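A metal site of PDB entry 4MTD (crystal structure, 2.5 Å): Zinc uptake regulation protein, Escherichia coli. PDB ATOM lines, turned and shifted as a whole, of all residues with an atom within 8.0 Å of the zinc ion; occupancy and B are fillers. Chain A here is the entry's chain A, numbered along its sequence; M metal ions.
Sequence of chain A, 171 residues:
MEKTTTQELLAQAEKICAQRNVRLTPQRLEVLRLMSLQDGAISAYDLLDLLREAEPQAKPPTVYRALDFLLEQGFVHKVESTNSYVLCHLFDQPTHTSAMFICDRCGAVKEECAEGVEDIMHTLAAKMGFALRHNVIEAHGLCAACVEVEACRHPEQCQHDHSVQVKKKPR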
ATOM      1  N   GLY A  74     -19.085 -17.640   7.709  1.00  0.00           N
ATOM      2  CA  GLY A  74     -19.997 -17.314   6.617  1.00  0.00           C
ATOM      3  C   GLY A  74     -19.378 -16.693   5.367  1.00  0.00           C
ATOM      4  O   GLY A  74     -20.115 -16.262   4.492  1.00  0.00           O
ATOM      5  N   PHE A  75     -18.046 -16.683   5.265  1.00  0.00           N
ATOM      6  CA  PHE A  75     -17.351 -15.732   4.371  1.00  0.00           C
ATOM      7  C   PHE A  75     -17.348 -16.058   2.884  1.00  0.00           C
ATOM      8  O   PHE A  75     -17.207 -15.142   2.074  1.00  0.00           O
ATOM      9  CB  PHE A  75     -15.912 -15.511   4.833  1.00  0.00           C
ATOM     10  CG  PHE A  75     -15.806 -15.020   6.240  1.00  0.00           C
ATOM     11  CD1 PHE A  75     -16.380 -13.822   6.605  1.00  0.00           C
ATOM     12  CD2 PHE A  75     -15.118 -15.748   7.192  1.00  0.00           C
ATOM     13  CE1 PHE A  75     -16.285 -13.359   7.901  1.00  0.00           C
ATOM     14  CE2 PHE A  75     -15.014 -15.282   8.488  1.00  0.00           C
ATOM     15  CZ  PHE A  75     -15.599 -14.083   8.844  1.00  0.00           C
ATOM     16  N   VAL A  76     -17.447 -17.340   2.516  1.00  0.00           N
ATOM     17  CA  VAL A  76     -17.485 -17.704   1.105  1.00  0.00           C
ATOM     18  C   VAL A  76     -18.525 -18.766   0.821  1.00  0.00           C
ATOM     19  O   VAL A  76     -18.956 -19.481   1.727  1.00  0.00           O
ATOM     20  CB  VAL A  76     -16.109 -18.181   0.569  1.00  0.00           C
ATOM     21  CG1 VAL A  76     -14.996 -17.231   0.979  1.00  0.00           C
ATOM     22  CG2 VAL A  76     -15.795 -19.598   1.010  1.00  0.00           C
ATOM     23  N   HIS A  77     -18.928 -18.853  -0.437  1.00  0.00           N
ATOM     24  CA  HIS A  77     -19.827 -19.890  -0.893  1.00  0.00           C
ATOM     25  C   HIS A  77     -19.164 -20.712  -1.971  1.00  0.00           C
ATOM     26  O   HIS A  77     -18.393 -20.171  -2.789  1.00  0.00           O
ATOM     27  CB  HIS A  77     -21.117 -19.296  -1.479  1.00  0.00           C
ATOM     28  CG  HIS A  77     -21.907 -18.461  -0.524  1.00  0.00           C
ATOM     29  ND1 HIS A  77     -22.463 -18.972   0.637  1.00  0.00           N
ATOM     30  CD2 HIS A  77     -22.267 -17.155  -0.567  1.00  0.00           C
ATOM     31  CE1 HIS A  77     -23.108 -18.011   1.267  1.00  0.00           C
ATOM     32  NE2 HIS A  77     -23.004 -16.904   0.563  1.00  0.00           N
ATOM     33  N   VAL A  86     -16.604 -18.084  -4.294  1.00  0.00           N
ATOM     34  CA  VAL A  86     -16.785 -16.642  -4.339  1.00  0.00           C
ATOM     35  C   VAL A  86     -17.032 -16.118  -2.930  1.00  0.00           C
ATOM     36  O   VAL A  86     -17.475 -16.861  -2.046  1.00  0.00           O
ATOM     37  CB  VAL A  86     -17.950 -16.276  -5.293  1.00  0.00           C
ATOM     38  CG1 VAL A  86     -19.283 -16.803  -4.767  1.00  0.00           C
ATOM     39  CG2 VAL A  86     -18.010 -14.773  -5.524  1.00  0.00           C
ATOM     40  N   LEU A  87     -16.718 -14.850  -2.706  1.00  0.00           N
ATOM     41  CA  LEU A  87     -17.055 -14.191  -1.455  1.00  0.00           C
ATOM     42  C   LEU A  87     -18.556 -14.054  -1.286  1.00  0.00           C
ATOM     43  O   LEU A  87     -19.271 -13.805  -2.248  1.00  0.00           O
ATOM     44  CB  LEU A  87     -16.469 -12.776  -1.384  1.00  0.00           C
ATOM     45  CG  LEU A  87     -15.058 -12.567  -0.869  1.00  0.00           C
ATOM     46  CD1 LEU A  87     -14.922 -11.092  -0.515  1.00  0.00           C
ATOM     47  CD2 LEU A  87     -14.763 -13.430   0.346  1.00  0.00           C
ATOM     48  N   CYS A  88     -19.021 -14.203  -0.054  1.00  0.00           N
ATOM     49  CA  CYS A  88     -20.390 -13.889   0.304  1.00  0.00           C
ATOM     50  C   CYS A  88     -20.522 -12.370   0.411  1.00  0.00           C
ATOM     51  O   CYS A  88     -19.675 -11.701   1.012  1.00  0.00           O
ATOM     52  CB  CYS A  88     -20.759 -14.548   1.640  1.00  0.00           C
ATOM     53  SG  CYS A  88     -22.329 -13.991   2.315  1.00  0.00           S
ATOM     54  N   HIS A  89     -21.589 -11.827  -0.171  1.00  0.00           N
ATOM     55  CA  HIS A  89     -21.784 -10.371  -0.230  1.00  0.00           C
ATOM     56  C   HIS A  89     -22.060  -9.675   1.120  1.00  0.00           C
ATOM     57  O   HIS A  89     -21.773  -8.489   1.264  1.00  0.00           O
ATOM     58  CB  HIS A  89     -22.870 -10.021  -1.267  1.00  0.00           C
ATOM     59  CG  HIS A  89     -24.270 -10.213  -0.776  1.00  0.00           C
ATOM     60  ND1 HIS A  89     -24.670 -11.308  -0.041  1.00  0.00           N
ATOM     61  CD2 HIS A  89     -25.386  -9.451  -0.949  1.00  0.00           C
ATOM     62  CE1 HIS A  89     -25.964 -11.207   0.231  1.00  0.00           C
ATOM     63  NE2 HIS A  89     -26.417 -10.093  -0.313  1.00  0.00           N
ATOM     64  N   LEU A  90     -22.613 -10.401   2.091  1.00  0.00           N
ATOM     65  CA  LEU A  90     -22.855  -9.858   3.442  1.00  0.00           C
ATOM     66  C   LEU A  90     -22.461 -10.871   4.530  1.00  0.00           C
ATOM     67  O   LEU A  90     -23.124 -11.892   4.687  1.00  0.00           O
ATOM     68  CB  LEU A  90     -24.329  -9.457   3.610  1.00  0.00           C
ATOM     69  CG  LEU A  90     -24.800  -9.060   5.021  1.00  0.00           C
ATOM     70  CD1 LEU A  90     -23.936  -7.947   5.605  1.00  0.00           C
ATOM     71  CD2 LEU A  90     -26.264  -8.648   5.015  1.00  0.00           C
ATOM     72  N   PHE A  91     -21.426 -10.569   5.302  1.00  0.00           N
ATOM     73  CA  PHE A  91     -20.820 -11.550   6.201  1.00  0.00           C
ATOM     74  C   PHE A  91     -21.665 -12.037   7.398  1.00  0.00           C
ATOM     75  O   PHE A  91     -22.256 -13.110   7.311  1.00  0.00           O
ATOM     76  CB  PHE A  91     -19.459 -11.062   6.709  1.00  0.00           C
ATOM     77  CG  PHE A  91     -18.369 -11.028   5.659  1.00  0.00           C
ATOM     78  CD1 PHE A  91     -18.442 -11.823   4.505  1.00  0.00           C
ATOM     79  CD2 PHE A  91     -17.248 -10.242   5.847  1.00  0.00           C
ATOM     80  CE1 PHE A  91     -17.438 -11.789   3.566  1.00  0.00           C
ATOM     81  CE2 PHE A  91     -16.243 -10.207   4.908  1.00  0.00           C
ATOM     82  CZ  PHE A  91     -16.333 -10.979   3.767  1.00  0.00           C
ATOM     83  N   GLN A  93     -24.272 -12.574   8.953  1.00  0.00           N
ATOM     84  CA  GLN A  93     -25.528 -13.340   8.990  1.00  0.00           C
ATOM     85  C   GLN A  93     -25.293 -14.864   9.091  1.00  0.00           C
ATOM     86  O   GLN A  93     -24.246 -15.360   8.675  1.00  0.00           O
ATOM     87  CB  GLN A  93     -26.375 -13.016   7.756  1.00  0.00           C
ATOM     88  CG  GLN A  93     -25.812 -13.553   6.446  1.00  0.00           C
ATOM     89  CD  GLN A  93     -26.509 -12.994   5.227  1.00  0.00           C
ATOM     90  OE1 GLN A  93     -26.182 -13.342   4.090  1.00  0.00           O
ATOM     91  NE2 GLN A  93     -27.489 -12.113   5.449  1.00  0.00           N
ATOM     92  N   PRO A  94     -26.275 -15.600   9.643  1.00  0.00           N
ATOM     93  CA  PRO A  94     -26.144 -17.055   9.799  1.00  0.00           C
ATOM     94  C   PRO A  94     -26.396 -17.835   8.508  1.00  0.00           C
ATOM     95  O   PRO A  94     -26.669 -17.238   7.465  1.00  0.00           O
ATOM     96  CB  PRO A  94     -27.218 -17.393  10.839  1.00  0.00           C
ATOM     97  CG  PRO A  94     -28.281 -16.378  10.589  1.00  0.00           C
ATOM     98  CD  PRO A  94     -27.569 -15.118  10.171  1.00  0.00           C
ATOM     99  N   THR A  95     -26.300 -19.166   8.582  1.00  0.00           N
ATOM    100  CA  THR A  95     -26.505 -20.047   7.427  1.00  0.00           C
ATOM    101  C   THR A  95     -27.773 -19.658   6.641  1.00  0.00           C
ATOM    102  O   THR A  95     -28.895 -19.802   7.133  1.00  0.00           O
ATOM    103  CB  THR A  95     -26.590 -21.525   7.844  1.00  0.00           C
ATOM    104  OG1 THR A  95     -27.184 -21.630   9.145  1.00  0.00           O
ATOM    105  CG2 THR A  95     -25.196 -22.161   7.886  1.00  0.00           C
ATOM    106  N   HIS A  96     -27.565 -19.165   5.425  1.00  0.00           N
ATOM    107  CA  HIS A  96     -28.632 -18.607   4.605  1.00  0.00           C
ATOM    108  C   HIS A  96     -28.672 -19.255   3.227  1.00  0.00           C
ATOM    109  O   HIS A  96     -27.640 -19.655   2.681  1.00  0.00           O
ATOM    110  CB  HIS A  96     -28.458 -17.090   4.463  1.00  0.00           C
ATOM    111  CG  HIS A  96     -27.134 -16.669   3.888  1.00  0.00           C
ATOM    112  ND1 HIS A  96     -25.988 -16.605   4.646  1.00  0.00           N
ATOM    113  CD2 HIS A  96     -26.784 -16.271   2.643  1.00  0.00           C
ATOM    114  CE1 HIS A  96     -24.982 -16.190   3.895  1.00  0.00           C
ATOM    115  NE2 HIS A  96     -25.440 -15.985   2.669  1.00  0.00           N
ATOM    116  N   THR A  97     -29.883 -19.360   2.670  1.00  0.00           N
ATOM    117  CA  THR A  97     -30.080 -19.789   1.292  1.00  0.00           C
ATOM    118  C   THR A  97     -30.180 -18.543   0.422  1.00  0.00           C
ATOM    119  O   THR A  97     -31.094 -17.741   0.588  1.00  0.00           O
ATOM    120  CB  THR A  97     -31.368 -20.651   1.155  1.00  0.00           C
ATOM    121  OG1 THR A  97     -31.124 -21.976   1.648  1.00  0.00           O
ATOM    122  CG2 THR A  97     -31.838 -20.751  -0.301  1.00  0.00           C
ATOM    123  N   SER A  98     -29.229 -18.398  -0.492  1.00  0.00           N
ATOM    124  CA  SER A  98     -29.205 -17.290  -1.453  1.00  0.00           C
ATOM    125  C   SER A  98     -29.251 -17.806  -2.890  1.00  0.00           C
ATOM    126  O   SER A  98     -28.760 -18.901  -3.187  1.00  0.00           O
ATOM    127  CB  SER A  98     -27.945 -16.440  -1.263  1.00  0.00           C
ATOM    128  OG  SER A  98     -28.146 -15.447  -0.272  1.00  0.00           O
ATOM    129  N   ALA A  99     -29.837 -17.001  -3.774  1.00  0.00           N
ATOM    130  CA  ALA A  99     -29.821 -17.266  -5.212  1.00  0.00           C
ATOM    131  C   ALA A  99     -28.561 -16.659  -5.826  1.00  0.00           C
ATOM    132  O   ALA A  99     -28.257 -15.500  -5.574  1.00  0.00           O
ATOM    133  CB  ALA A  99     -31.058 -16.704  -5.865  1.00  0.00           C
ATOM    134  N   MET A 100     -27.842 -17.438  -6.635  1.00  0.00           N
ATOM    135  CA  MET A 100     -26.556 -16.995  -7.206  1.00  0.00           C
ATOM    136  C   MET A 100     -26.713 -16.808  -8.699  1.00  0.00           C
ATOM    137  O   MET A 100     -27.031 -17.749  -9.414  1.00  0.00           O
ATOM    138  CB  MET A 100     -25.454 -18.035  -6.950  1.00  0.00           C
ATOM    139  CG  MET A 100     -25.250 -18.452  -5.503  1.00  0.00           C
ATOM    140  SD  MET A 100     -23.608 -18.080  -4.829  1.00  0.00           S
ATOM    141  CE  MET A 100     -23.861 -16.427  -4.188  1.00  0.00           C
ATOM    142  N   GLU A 111     -25.192 -12.159  -5.501  1.00  0.00           N
ATOM    143  CA  GLU A 111     -25.914 -12.949  -4.505  1.00  0.00           C
ATOM    144  C   GLU A 111     -27.208 -12.213  -4.136  1.00  0.00           C
ATOM    145  O   GLU A 111     -27.156 -11.096  -3.629  1.00  0.00           O
ATOM    146  CB  GLU A 111     -25.032 -13.179  -3.276  1.00  0.00           C
ATOM    147  CG  GLU A 111     -25.622 -14.172  -2.281  1.00  0.00           C
ATOM    148  CD  GLU A 111     -24.799 -14.382  -1.013  1.00  0.00           C
ATOM    149  OE1 GLU A 111     -25.363 -14.996  -0.088  1.00  0.00           O
ATOM    150  OE2 GLU A 111     -23.624 -13.954  -0.910  1.00  0.00           O
ATOM    151  N   GLU A 112     -28.358 -12.827  -4.406  1.00  0.00           N
ATOM    152  CA  GLU A 112     -29.663 -12.230  -4.089  1.00  0.00           C
ATOM    153  C   GLU A 112     -30.445 -13.098  -3.135  1.00  0.00           C
ATOM    154  O   GLU A 112     -30.180 -14.296  -2.996  1.00  0.00           O
ATOM    155  CB  GLU A 112     -30.495 -12.023  -5.358  1.00  0.00           C
ATOM    156  CG  GLU A 112     -29.892 -11.039  -6.348  1.00  0.00           C
ATOM    157  CD  GLU A 112     -30.519  -9.647  -6.284  1.00  0.00           C
ATOM    158  OE1 GLU A 112     -31.740  -9.517  -6.530  1.00  0.00           O
ATOM    159  OE2 GLU A 112     -29.776  -8.672  -6.028  1.00  0.00           O
HETATM  160 ZN    ZN M   1     -23.993 -15.268   1.329  1.00  0.00          ZN
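The backbone carbonyl oxygen (O) of Leu 90 sits close to the side-chain sulfur (SG) of Cys 88 (3.3 Å).
The backbone NH of His 77 sits at hydrogen-bond distance from the backbone carbonyl oxygen of Val 86.
A ring nitrogen (ND1) of His 96 lies within hydrogen-bond range of the backbone carbonyl oxygen (O) of Pro 94 (3.0 Å).
ND1 of His 96 lies close to OE1 of Gln 93, at 3.3 Å.
The side-chain carboxylate of Glu 111 lies close to the side-chain hydroxyl of Ser 98 (2.8 Å).
The backbone NH (N) of Cys 88 is in hydrogen-bond range of the backbone carbonyl oxygen (O) of Phe 75, 2.9 Å away.
The side-chain carboxylate (OE2) of Glu 111 sits at hydrogen-bond distance from a ring nitrogen (ND1) of His 89.
Within 4 Å of the zinc ion: His 77, Cys 88, His 96 and Glu 111.
The nearest printed residue that does not touch the zinc ion is Gln 93 (4.02 Å).
OE1 of Glu 111 is bound to the zinc ion (2.0 Å).
NE2 of His 77 binds the zinc ion, 2.1 Å away.
NE2 of His 96 is bound to the zinc ion (2.1 Å).
The zinc ion is bound by the side-chain sulfur (SG) of Cys 88 (2.3 Å).
The zinc ion has four donor atoms within binding distance.
Slightly farther from the zinc ion lies the side-chain carboxylate (OE2) of Glu 111 (2.6 Å).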
